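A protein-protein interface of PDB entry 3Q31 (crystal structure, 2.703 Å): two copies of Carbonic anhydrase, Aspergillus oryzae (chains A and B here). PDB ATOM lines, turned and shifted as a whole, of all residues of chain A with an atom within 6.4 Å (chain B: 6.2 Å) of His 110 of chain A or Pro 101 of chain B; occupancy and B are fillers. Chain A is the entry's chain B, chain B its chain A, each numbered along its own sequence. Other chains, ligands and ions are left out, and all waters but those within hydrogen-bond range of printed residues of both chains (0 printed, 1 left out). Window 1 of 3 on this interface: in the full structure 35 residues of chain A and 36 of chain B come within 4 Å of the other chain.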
ATOM      1  N   PRO A 101       5.286   0.441   8.685  1.00  0.00           N
ATOM      2  CA  PRO A 101       6.447  -0.345   9.116  1.00  0.00           C
ATOM      3  C   PRO A 101       7.135  -0.993   7.931  1.00  0.00           C
ATOM      4  O   PRO A 101       6.713  -0.797   6.792  1.00  0.00           O
ATOM      5  CB  PRO A 101       5.804  -1.452   9.944  1.00  0.00           C
ATOM      6  CG  PRO A 101       4.432  -1.600   9.352  1.00  0.00           C
ATOM      7  CD  PRO A 101       4.037  -0.173   9.172  1.00  0.00           C
ATOM      8  N   SER A 102       8.170  -1.781   8.194  1.00  0.00           N
ATOM      9  CA  SER A 102       8.821  -2.501   7.112  1.00  0.00           C
ATOM     10  C   SER A 102       7.807  -3.407   6.465  1.00  0.00           C
ATOM     11  O   SER A 102       6.747  -3.672   7.009  1.00  0.00           O
ATOM     12  CB  SER A 102       9.983  -3.337   7.635  1.00  0.00           C
ATOM     13  OG  SER A 102       9.495  -4.466   8.324  1.00  0.00           O
ATOM     14  N   HIS A 104       9.004  -6.403   4.626  1.00  0.00           N
ATOM     15  CA  HIS A 104       9.565  -7.718   4.879  1.00  0.00           C
ATOM     16  C   HIS A 104       9.704  -7.903   6.380  1.00  0.00           C
ATOM     17  O   HIS A 104       9.685  -6.928   7.130  1.00  0.00           O
ATOM     18  CB  HIS A 104      10.930  -7.878   4.217  1.00  0.00           C
ATOM     19  CG  HIS A 104      10.869  -8.021   2.725  1.00  0.00           C
ATOM     20  ND1 HIS A 104      10.773  -6.943   1.869  1.00  0.00           N
ATOM     21  CD2 HIS A 104      10.914  -9.119   1.934  1.00  0.00           C
ATOM     22  CE1 HIS A 104      10.744  -7.373   0.621  1.00  0.00           C
ATOM     23  NE2 HIS A 104      10.832  -8.690   0.632  1.00  0.00           N
ATOM     24  N   HIS A 105       9.829  -9.157   6.804  1.00  0.00           N
ATOM     25  CA  HIS A 105      10.167  -9.501   8.179  1.00  0.00           C
ATOM     26  C   HIS A 105      11.315 -10.496   8.124  1.00  0.00           C
ATOM     27  O   HIS A 105      11.424 -11.260   7.171  1.00  0.00           O
ATOM     28  CB  HIS A 105       8.977 -10.156   8.928  1.00  0.00           C
ATOM     29  CG  HIS A 105       7.743  -9.310   8.992  1.00  0.00           C
ATOM     30  ND1 HIS A 105       6.483  -9.845   9.151  1.00  0.00           N
ATOM     31  CD2 HIS A 105       7.574  -7.968   8.918  1.00  0.00           C
ATOM     32  CE1 HIS A 105       5.594  -8.867   9.179  1.00  0.00           C
ATOM     33  NE2 HIS A 105       6.229  -7.717   9.030  1.00  0.00           N
ATOM     34  N   VAL A 106      12.147 -10.514   9.156  1.00  0.00           N
ATOM     35  CA  VAL A 106      13.222 -11.495   9.242  1.00  0.00           C
ATOM     36  C   VAL A 106      13.034 -12.404  10.456  1.00  0.00           C
ATOM     37  O   VAL A 106      12.949 -11.932  11.604  1.00  0.00           O
ATOM     38  CB  VAL A 106      14.609 -10.822   9.327  1.00  0.00           C
ATOM     39  CG1 VAL A 106      15.696 -11.838   9.033  1.00  0.00           C
ATOM     40  CG2 VAL A 106      14.695  -9.654   8.375  1.00  0.00           C
ATOM     41  N   GLU A 108      10.495 -13.722  11.230  1.00  0.00           N
ATOM     42  CA  GLU A 108       9.208 -13.162  11.648  1.00  0.00           C
ATOM     43  C   GLU A 108       9.203 -11.774  12.260  1.00  0.00           C
ATOM     44  O   GLU A 108       8.119 -11.221  12.486  1.00  0.00           O
ATOM     45  CB  GLU A 108       8.408 -14.126  12.502  1.00  0.00           C
ATOM     46  CG  GLU A 108       7.450 -14.935  11.685  1.00  0.00           C
ATOM     47  CD  GLU A 108       8.098 -16.182  11.110  1.00  0.00           C
ATOM     48  OE1 GLU A 108       9.076 -16.690  11.710  1.00  0.00           O
ATOM     49  OE2 GLU A 108       7.626 -16.662  10.058  1.00  0.00           O
ATOM     50  N   GLU A 109      10.384 -11.208  12.512  1.00  0.00           N
ATOM     51  CA  GLU A 109      10.460  -9.888  13.152  1.00  0.00           C
ATOM     52  C   GLU A 109      10.352  -8.726  12.153  1.00  0.00           C
ATOM     53  O   GLU A 109      11.096  -8.659  11.179  1.00  0.00           O
ATOM     54  CB  GLU A 109      11.735  -9.728  13.995  1.00  0.00           C
ATOM     55  CG  GLU A 109      11.740  -8.438  14.793  1.00  0.00           C
ATOM     56  CD  GLU A 109      12.991  -8.239  15.628  1.00  0.00           C
ATOM     57  OE1 GLU A 109      13.141  -7.130  16.200  1.00  0.00           O
ATOM     58  OE2 GLU A 109      13.822  -9.174  15.714  1.00  0.00           O
ATOM     59  N   HIS A 110       9.426  -7.810  12.401  1.00  0.00           N
ATOM     60  CA  HIS A 110       9.308  -6.644  11.551  1.00  0.00           C
ATOM     61  C   HIS A 110      10.225  -5.539  12.047  1.00  0.00           C
ATOM     62  O   HIS A 110      10.880  -5.681  13.094  1.00  0.00           O
ATOM     63  CB  HIS A 110       7.862  -6.152  11.492  1.00  0.00           C
ATOM     64  CG  HIS A 110       7.466  -5.286  12.648  1.00  0.00           C
ATOM     65  ND1 HIS A 110       7.220  -5.787  13.906  1.00  0.00           N
ATOM     66  CD2 HIS A 110       7.241  -3.954  12.728  1.00  0.00           C
ATOM     67  CE1 HIS A 110       6.877  -4.802  14.717  1.00  0.00           C
ATOM     68  NE2 HIS A 110       6.877  -3.679  14.025  1.00  0.00           N
ATOM     69  N   PHE A 111      10.276  -4.449  11.280  1.00  0.00           N
ATOM     70  CA  PHE A 111      11.060  -3.279  11.657  1.00  0.00           C
ATOM     71  C   PHE A 111      10.250  -2.042  11.422  1.00  0.00           C
ATOM     72  O   PHE A 111       9.326  -2.045  10.593  1.00  0.00           O
ATOM     73  CB  PHE A 111      12.342  -3.207  10.847  1.00  0.00           C
ATOM     74  CG  PHE A 111      13.270  -4.354  11.098  1.00  0.00           C
ATOM     75  CD1 PHE A 111      13.122  -5.541  10.409  1.00  0.00           C
ATOM     76  CD2 PHE A 111      14.283  -4.248  12.040  1.00  0.00           C
ATOM     77  CE1 PHE A 111      13.969  -6.595  10.641  1.00  0.00           C
ATOM     78  CE2 PHE A 111      15.129  -5.303  12.279  1.00  0.00           C
ATOM     79  CZ  PHE A 111      14.973  -6.480  11.580  1.00  0.00           C
ATOM     80  N   PRO A 112      10.603  -0.966  12.134  1.00  0.00           N
ATOM     81  CA  PRO A 112       9.863   0.298  12.040  1.00  0.00           C
ATOM     82  C   PRO A 112       9.872   0.867  10.622  1.00  0.00           C
ATOM     83  O   PRO A 112       8.891   1.515  10.262  1.00  0.00           O
ATOM     84  CB  PRO A 112      10.640   1.233  12.966  1.00  0.00           C
ATOM     85  CG  PRO A 112      12.012   0.635  13.078  1.00  0.00           C
ATOM     86  CD  PRO A 112      11.829  -0.844  12.947  1.00  0.00           C
ATOM     87  N   PHE A 133      15.440  -0.586   8.783  1.00  0.00           N
ATOM     88  CA  PHE A 133      15.791   0.368   9.822  1.00  0.00           C
ATOM     89  C   PHE A 133      15.506  -0.190  11.202  1.00  0.00           C
ATOM     90  O   PHE A 133      14.492  -0.859  11.407  1.00  0.00           O
ATOM     91  CB  PHE A 133      15.017   1.670   9.631  1.00  0.00           C
ATOM     92  CG  PHE A 133      15.538   2.511   8.502  1.00  0.00           C
ATOM     93  CD1 PHE A 133      16.647   3.330   8.683  1.00  0.00           C
ATOM     94  CD2 PHE A 133      14.931   2.477   7.253  1.00  0.00           C
ATOM     95  CE1 PHE A 133      17.131   4.101   7.649  1.00  0.00           C
ATOM     96  CE2 PHE A 133      15.401   3.244   6.225  1.00  0.00           C
ATOM     97  CZ  PHE A 133      16.512   4.056   6.413  1.00  0.00           C
ATOM     98  N   GLN A 134      16.372   0.102  12.164  1.00  0.00           N
ATOM     99  CA  GLN A 134      16.076  -0.248  13.550  1.00  0.00           C
ATOM    100  C   GLN A 134      16.330   0.920  14.488  1.00  0.00           C
ATOM    101  O   GLN A 134      17.400   1.513  14.444  1.00  0.00           O
ATOM    102  CB  GLN A 134      16.915  -1.440  13.991  1.00  0.00           C
ATOM    103  CG  GLN A 134      16.671  -1.838  15.416  1.00  0.00           C
ATOM    104  CD  GLN A 134      15.404  -2.619  15.563  1.00  0.00           C
ATOM    105  OE1 GLN A 134      15.455  -3.826  15.760  1.00  0.00           O
ATOM    106  NE2 GLN A 134      14.250  -1.941  15.462  1.00  0.00           N
ATOM    107  N   TYR A 213      11.762   8.750  12.834  1.00  0.00           N
ATOM    108  CA  TYR A 213      10.676   7.759  12.761  1.00  0.00           C
ATOM    109  C   TYR A 213       9.290   8.398  12.880  1.00  0.00           C
ATOM    110  O   TYR A 213       8.378   8.121  12.080  1.00  0.00           O
ATOM    111  CB  TYR A 213      10.839   6.688  13.854  1.00  0.00           C
ATOM    112  CG  TYR A 213       9.690   5.675  13.962  1.00  0.00           C
ATOM    113  CD1 TYR A 213       9.526   4.675  13.012  1.00  0.00           C
ATOM    114  CD2 TYR A 213       8.792   5.702  15.036  1.00  0.00           C
ATOM    115  CE1 TYR A 213       8.508   3.740  13.102  1.00  0.00           C
ATOM    116  CE2 TYR A 213       7.753   4.760  15.141  1.00  0.00           C
ATOM    117  CZ  TYR A 213       7.621   3.777  14.162  1.00  0.00           C
ATOM    118  OH  TYR A 213       6.607   2.818  14.209  1.00  0.00           O
ATOM    119  N   TYR A 222       0.764   4.697   7.149  1.00  0.00           N
ATOM    120  CA  TYR A 222       0.957   3.264   7.161  1.00  0.00           C
ATOM    121  C   TYR A 222       0.920   2.884   5.706  1.00  0.00           C
ATOM    122  O   TYR A 222       0.012   3.302   4.978  1.00  0.00           O
ATOM    123  CB  TYR A 222      -0.172   2.544   7.908  1.00  0.00           C
ATOM    124  CG  TYR A 222      -0.026   1.030   7.844  1.00  0.00           C
ATOM    125  CD1 TYR A 222      -0.697   0.288   6.896  1.00  0.00           C
ATOM    126  CD2 TYR A 222       0.834   0.356   8.711  1.00  0.00           C
ATOM    127  CE1 TYR A 222      -0.536  -1.101   6.818  1.00  0.00           C
ATOM    128  CE2 TYR A 222       1.006  -1.019   8.641  1.00  0.00           C
ATOM    129  CZ  TYR A 222       0.321  -1.744   7.692  1.00  0.00           C
ATOM    130  OH  TYR A 222       0.494  -3.111   7.627  1.00  0.00           O
ATOM    131  N   HIS B  99       0.607  -5.820  21.391  1.00  0.00           N
ATOM    132  CA  HIS B  99       0.768  -6.010  19.967  1.00  0.00           C
ATOM    133  C   HIS B  99       1.776  -5.009  19.438  1.00  0.00           C
ATOM    134  O   HIS B  99       1.807  -3.828  19.836  1.00  0.00           O
ATOM    135  CB  HIS B  99      -0.539  -5.739  19.255  1.00  0.00           C
ATOM    136  CG  HIS B  99      -1.610  -6.735  19.544  1.00  0.00           C
ATOM    137  ND1 HIS B  99      -1.722  -7.921  18.850  1.00  0.00           N
ATOM    138  CD2 HIS B  99      -2.643  -6.702  20.413  1.00  0.00           C
ATOM    139  CE1 HIS B  99      -2.775  -8.582  19.292  1.00  0.00           C
ATOM    140  NE2 HIS B  99      -3.348  -7.867  20.242  1.00  0.00           N
ATOM    141  N   THR B 100       2.585  -5.485  18.516  1.00  0.00           N
ATOM    142  CA  THR B 100       3.559  -4.642  17.866  1.00  0.00           C
ATOM    143  C   THR B 100       3.691  -5.089  16.399  1.00  0.00           C
ATOM    144  O   THR B 100       4.030  -6.251  16.142  1.00  0.00           O
ATOM    145  CB  THR B 100       4.901  -4.730  18.603  1.00  0.00           C
ATOM    146  OG1 THR B 100       5.764  -3.712  18.114  1.00  0.00           O
ATOM    147  CG2 THR B 100       5.554  -6.052  18.376  1.00  0.00           C
ATOM    148  N   PRO B 101       3.382  -4.192  15.434  1.00  0.00           N
ATOM    149  CA  PRO B 101       2.891  -2.813  15.612  1.00  0.00           C
ATOM    150  C   PRO B 101       1.488  -2.785  16.178  1.00  0.00           C
ATOM    151  O   PRO B 101       0.889  -3.840  16.388  1.00  0.00           O
ATOM    152  CB  PRO B 101       2.806  -2.286  14.171  1.00  0.00           C
ATOM    153  CG  PRO B 101       2.606  -3.520  13.330  1.00  0.00           C
ATOM    154  CD  PRO B 101       3.529  -4.521  14.001  1.00  0.00           C
ATOM    155  N   SER B 102       0.950  -1.593  16.386  1.00  0.00           N
ATOM    156  CA  SER B 102      -0.429  -1.488  16.814  1.00  0.00           C
ATOM    157  C   SER B 102      -1.309  -2.201  15.805  1.00  0.00           C
ATOM    158  O   SER B 102      -0.888  -2.473  14.683  1.00  0.00           O
ATOM    159  CB  SER B 102      -0.851  -0.027  16.926  1.00  0.00           C
ATOM    160  OG  SER B 102      -1.102   0.510  15.650  1.00  0.00           O
ATOM    161  N   GLU B 103      -2.540  -2.502  16.189  1.00  0.00           N
ATOM    162  CA  GLU B 103      -3.450  -3.183  15.282  1.00  0.00           C
ATOM    163  C   GLU B 103      -4.390  -2.159  14.696  1.00  0.00           C
ATOM    164  O   GLU B 103      -4.614  -2.145  13.486  1.00  0.00           O
ATOM    165  CB  GLU B 103      -4.223  -4.284  16.005  1.00  0.00           C
ATOM    166  CG  GLU B 103      -3.342  -5.333  16.646  1.00  0.00           C
ATOM    167  CD  GLU B 103      -4.046  -6.658  16.781  1.00  0.00           C
ATOM    168  OE1 GLU B 103      -4.727  -6.882  17.805  1.00  0.00           O
ATOM    169  OE2 GLU B 103      -3.922  -7.476  15.852  1.00  0.00           O
ATOM    170  N   HIS B 110      -0.496   4.344  11.999  1.00  0.00           N
ATOM    171  CA  HIS B 110      -0.292   3.260  12.952  1.00  0.00           C
ATOM    172  C   HIS B 110       0.635   3.705  14.091  1.00  0.00           C
ATOM    173  O   HIS B 110       1.130   4.839  14.104  1.00  0.00           O
ATOM    174  CB  HIS B 110       0.273   2.032  12.241  1.00  0.00           C
ATOM    175  CG  HIS B 110       1.752   2.091  12.016  1.00  0.00           C
ATOM    176  ND1 HIS B 110       2.324   2.866  11.030  1.00  0.00           N
ATOM    177  CD2 HIS B 110       2.776   1.467  12.650  1.00  0.00           C
ATOM    178  CE1 HIS B 110       3.638   2.718  11.072  1.00  0.00           C
ATOM    179  NE2 HIS B 110       3.940   1.872  12.042  1.00  0.00           N
ATOM    180  N   PHE B 111       0.859   2.815  15.052  1.00  0.00           N
ATOM    181  CA  PHE B 111       1.759   3.094  16.173  1.00  0.00           C
ATOM    182  C   PHE B 111       2.620   1.879  16.439  1.00  0.00           C
ATOM    183  O   PHE B 111       2.261   0.757  16.086  1.00  0.00           O
ATOM    184  CB  PHE B 111       0.973   3.459  17.432  1.00  0.00           C
ATOM    185  CG  PHE B 111       0.178   4.713  17.295  1.00  0.00           C
ATOM    186  CD1 PHE B 111      -1.095   4.684  16.761  1.00  0.00           C
ATOM    187  CD2 PHE B 111       0.722   5.941  17.667  1.00  0.00           C
ATOM    188  CE1 PHE B 111      -1.823   5.858  16.616  1.00  0.00           C
ATOM    189  CE2 PHE B 111       0.007   7.119  17.525  1.00  0.00           C
ATOM    190  CZ  PHE B 111      -1.264   7.078  17.002  1.00  0.00           C
ATOM    191  N   PRO B 112       3.764   2.097  17.068  1.00  0.00           N
ATOM    192  CA  PRO B 112       4.722   1.017  17.271  1.00  0.00           C
ATOM    193  C   PRO B 112       4.142  -0.061  18.183  1.00  0.00           C
ATOM    194  O   PRO B 112       4.521  -1.220  18.028  1.00  0.00           O
ATOM    195  CB  PRO B 112       5.908   1.720  17.933  1.00  0.00           C
ATOM    196  CG  PRO B 112       5.315   2.940  18.547  1.00  0.00           C
ATOM    197  CD  PRO B 112       4.204   3.363  17.656  1.00  0.00           C
ATOM    198  N   MET B 113       3.230   0.301  19.091  1.00  0.00           N
ATOM    199  CA  MET B 113       2.674  -0.671  20.036  1.00  0.00           C
ATOM    200  C   MET B 113       1.250  -0.394  20.501  1.00  0.00           C
ATOM    201  O   MET B 113       0.840   0.760  20.636  1.00  0.00           O
ATOM    202  CB  MET B 113       3.581  -0.800  21.264  1.00  0.00           C
ATOM    203  CG  MET B 113       3.371  -2.088  22.065  1.00  0.00           C
ATOM    204  SD  MET B 113       4.808  -2.477  23.094  1.00  0.00           S
ATOM    205  CE  MET B 113       4.825  -0.958  24.034  1.00  0.00           C
ATOM    206  N   GLU B 114       0.521  -1.475  20.794  1.00  0.00           N
ATOM    207  CA  GLU B 114      -0.822  -1.384  21.363  1.00  0.00           C
ATOM    208  C   GLU B 114      -0.988  -2.368  22.531  1.00  0.00           C
ATOM    209  O   GLU B 114      -0.562  -3.519  22.406  1.00  0.00           O
ATOM    210  CB  GLU B 114      -1.844  -1.680  20.266  1.00  0.00           C
ATOM    211  CG  GLU B 114      -3.277  -1.365  20.628  1.00  0.00           C
ATOM    212  CD  GLU B 114      -4.209  -1.416  19.428  1.00  0.00           C
ATOM    213  OE1 GLU B 114      -3.758  -1.198  18.279  1.00  0.00           O
ATOM    214  OE2 GLU B 114      -5.412  -1.653  19.632  1.00  0.00           O
ATOM    215  N   TYR B 213      10.741  -0.697  23.307  1.00  0.00           N
ATOM    216  CA  TYR B 213      10.193  -1.087  22.001  1.00  0.00           C
ATOM    217  C   TYR B 213      10.988  -2.211  21.370  1.00  0.00           C
ATOM    218  O   TYR B 213      10.427  -3.182  20.880  1.00  0.00           O
ATOM    219  CB  TYR B 213      10.201   0.102  21.052  1.00  0.00           C
ATOM    220  CG  TYR B 213       9.816  -0.205  19.605  1.00  0.00           C
ATOM    221  CD1 TYR B 213       8.485  -0.422  19.251  1.00  0.00           C
ATOM    222  CD2 TYR B 213      10.770  -0.217  18.585  1.00  0.00           C
ATOM    223  CE1 TYR B 213       8.116  -0.662  17.933  1.00  0.00           C
ATOM    224  CE2 TYR B 213      10.403  -0.466  17.263  1.00  0.00           C
ATOM    225  CZ  TYR B 213       9.081  -0.681  16.954  1.00  0.00           C
ATOM    226  OH  TYR B 213       8.713  -0.936  15.671  1.00  0.00           O
ATOM    227  N   LYS B 217       9.638  -5.976  20.722  1.00  0.00           N
ATOM    228  CA  LYS B 217       9.600  -6.329  19.300  1.00  0.00           C
ATOM    229  C   LYS B 217      10.363  -7.604  19.013  1.00  0.00           C
ATOM    230  O   LYS B 217       9.916  -8.435  18.241  1.00  0.00           O
ATOM    231  CB  LYS B 217      10.172  -5.198  18.431  1.00  0.00           C
ATOM    232  CG  LYS B 217       9.904  -5.374  16.933  1.00  0.00           C
ATOM    233  CD  LYS B 217      10.079  -4.085  16.125  1.00  0.00           C
ATOM    234  CE  LYS B 217      11.530  -3.724  16.061  1.00  0.00           C
ATOM    235  NZ  LYS B 217      12.318  -4.806  15.387  1.00  0.00           N
ATOM    236  N   LYS B 221       8.011 -10.251  17.883  1.00  0.00           N
ATOM    237  CA  LYS B 221       8.318 -10.328  16.442  1.00  0.00           C
ATOM    238  C   LYS B 221       7.382  -9.512  15.541  1.00  0.00           C
ATOM    239  O   LYS B 221       7.789  -8.502  14.980  1.00  0.00           O
ATOM    240  CB  LYS B 221       8.435 -11.781  15.973  1.00  0.00           C
ATOM    241  CG  LYS B 221       9.663 -12.458  16.520  1.00  0.00           C
ATOM    242  CD  LYS B 221       9.546 -13.963  16.471  1.00  0.00           C
ATOM    243  CE  LYS B 221      10.902 -14.602  16.742  1.00  0.00           C
ATOM    244  NZ  LYS B 221      11.521 -14.061  17.989  1.00  0.00           N
ATOM    245  N   TYR B 222       6.144  -9.966  15.396  1.00  0.00           N
ATOM    246  CA  TYR B 222       5.112  -9.234  14.677  1.00  0.00           C
ATOM    247  C   TYR B 222       3.851  -9.997  15.002  1.00  0.00           C
ATOM    248  O   TYR B 222       3.835 -11.224  14.904  1.00  0.00           O
ATOM    249  CB  TYR B 222       5.342  -9.235  13.160  1.00  0.00           C
ATOM    250  CG  TYR B 222       4.227  -8.553  12.393  1.00  0.00           C
ATOM    251  CD1 TYR B 222       3.191  -9.283  11.821  1.00  0.00           C
ATOM    252  CD2 TYR B 222       4.191  -7.172  12.273  1.00  0.00           C
ATOM    253  CE1 TYR B 222       2.159  -8.649  11.131  1.00  0.00           C
ATOM    254  CE2 TYR B 222       3.164  -6.528  11.588  1.00  0.00           C
ATOM    255  CZ  TYR B 222       2.150  -7.267  11.014  1.00  0.00           C
ATOM    256  OH  TYR B 222       1.139  -6.606  10.326  1.00  0.00           O
ATOM    257  N   ASN B 223       2.810  -9.285  15.420  1.00  0.00           N
ATOM    258  CA  ASN B 223       1.581  -9.946  15.828  1.00  0.00           C
ATOM    259  C   ASN B 223       0.344  -9.083  15.655  1.00  0.00           C
ATOM    260  O   ASN B 223      -0.506  -9.022  16.532  1.00  0.00           O
ATOM    261  CB  ASN B 223       1.689 -10.434  17.274  1.00  0.00           C
ATOM    262  CG  ASN B 223       1.582  -9.305  18.292  1.00  0.00           C
ATOM    263  OD1 ASN B 223       1.750  -8.132  17.963  1.00  0.00           O
ATOM    264  ND2 ASN B 223       1.298  -9.663  19.543  1.00  0.00           N
ATOM    265  N   ALA B 224       0.238  -8.411  14.519  1.00  0.00           N
ATOM    266  CA  ALA B 224      -0.904  -7.550  14.292  1.00  0.00           C
ATOM    267  C   ALA B 224      -1.723  -8.037  13.121  1.00  0.00           C
ATOM    268  O   ALA B 224      -1.187  -8.365  12.068  1.00  0.00           O
ATOM    269  CB  ALA B 224      -0.461  -6.127  14.077  1.00  0.00           C
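The side-chain carboxylate (OE1) of Glu 109 of chain A lies within salt-bridge range of the side-chain amino group (NZ) of Lys 217 of chain B (2.6 Å).
The side-chain amino group of Lys 217 of chain B lies within hydrogen-bond range of the backbone carbonyl oxygen of His 110 of chain A (2.8 Å).
The side-chain amide oxygen (OE1) of Gln 134 of chain A lies within hydrogen-bond range of the side-chain amino group (NZ) of Lys 217 of chain B, at 3.3 Å.
A ring nitrogen (ND1) of His 110 of chain A sits at hydrogen-bond distance from the backbone carbonyl oxygen of Lys 221 of chain B.
The backbone carbonyl oxygen (O) of Pro 112 of chain B is in hydrogen-bond range of the side-chain hydroxyl (OG1) of Thr 100 of chain B (2.8 Å).
The side-chain amide oxygen (OD1) of Asn 223 of chain B lies within hydrogen-bond range of the backbone NH (N) of Thr 100 of chain B, at 2.8 Å.
O of Ala 224 of chain B is in hydrogen-bond range of OH of Tyr 222 of chain B (3.4 Å).
The backbone NH (N) of Ser 102 of chain A lies within hydrogen-bond range of the backbone carbonyl oxygen (O) of Phe 111 of chain A (2.7 Å).
Pro 101 of chain A touches His 110 of chain B.
CE1 of His 105 of chain A touches CG of Tyr 222 of chain B (3.5 Å).
Glu 108 of chain A touches Lys 221 of chain B (O to CB, 3.5 Å).
Glu 109 of chain A touches Lys 221 of chain B.
His 110 of chain A touches Tyr 213 of chain B (NE2 to OH, 3.7 Å).
CD2 of Tyr 222 of chain B touches ND1 of His 110 of chain A (3.7 Å).
Phe 111 of chain A touches Lys 217 of chain B (CD2 to NZ, 3.9 Å).
OH of Tyr 213 of chain B touches CB of Pro 112 of chain A, 3.97 Å away.
His 110 of chain B touches Tyr 213 of chain A (NE2 to OH, 3.6 Å).
Tyr 222 of chain A touches His 110 of chain B.
His 110 of chain A touches just these residues of chain B: Thr 100 (3.5 Å), Pro 101 (3.4 Å), Tyr 213 (3.7 Å), Lys 217 (2.8 Å), Lys 221 (3.0 Å) and Tyr 222 (3.7 Å).
Of the printed residues of chain B, His 105 of chain A touches Tyr 222.
Printed residues of chain B within 4 Å of Pro 112 of chain A: Tyr 213.
Printed residues of chain B within 4 Å of Gln 134 of chain A: Lys 217.
Ala 224 of chain B touches none of the printed residues of chain A.
The nearest residue of chain B that does not touch His 110 of chain A is Pro 112 of chain B (5.3 Å).
The nearest residue of chain A that does not touch Pro 101 of chain B is Pro 101 of chain A (4.8 Å).
The nearest printed residue of chain A that does not touch Lys 221 of chain B is Val 106 of chain A (5.9 Å).
Of the 16 printed residues of chain B, 8 touch a printed residue of chain A.
Hydrophobic or aromatic side chains of chain B that line the printed part of chain A: Pro 101, His 110, Pro 112, Tyr 213 and Tyr 222.
Along chain A the printed residues that touch a printed residue of chain B span positions 101 to 222.
Among the printed residues, Asp or Glu carboxylates within 4 Å of a Lys or Arg side-chain nitrogen of the other chain: Glu 109 of chain A with Lys 217 of chain B.
Pro 101 of chain A touches His 110 of chain B, and with the chains exchanged His 110 of chain A touches Pro 101 of chain B.
His 110 of chain A touches Tyr 213 of chain B, and with the chains exchanged Tyr 213 of chain A touches His 110 of chain B.
His 110 of chain A touches Tyr 222 of chain B, and with the chains exchanged Tyr 222 of chain A touches His 110 of chain B.
Pro 112 of chain A touches Tyr 213 of chain B, and with the chains exchanged Tyr 213 of chain A touches Pro 112 of chain B.
Positions printed for both chains: 101, 102, 110, 111, 112, 213 and 222.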
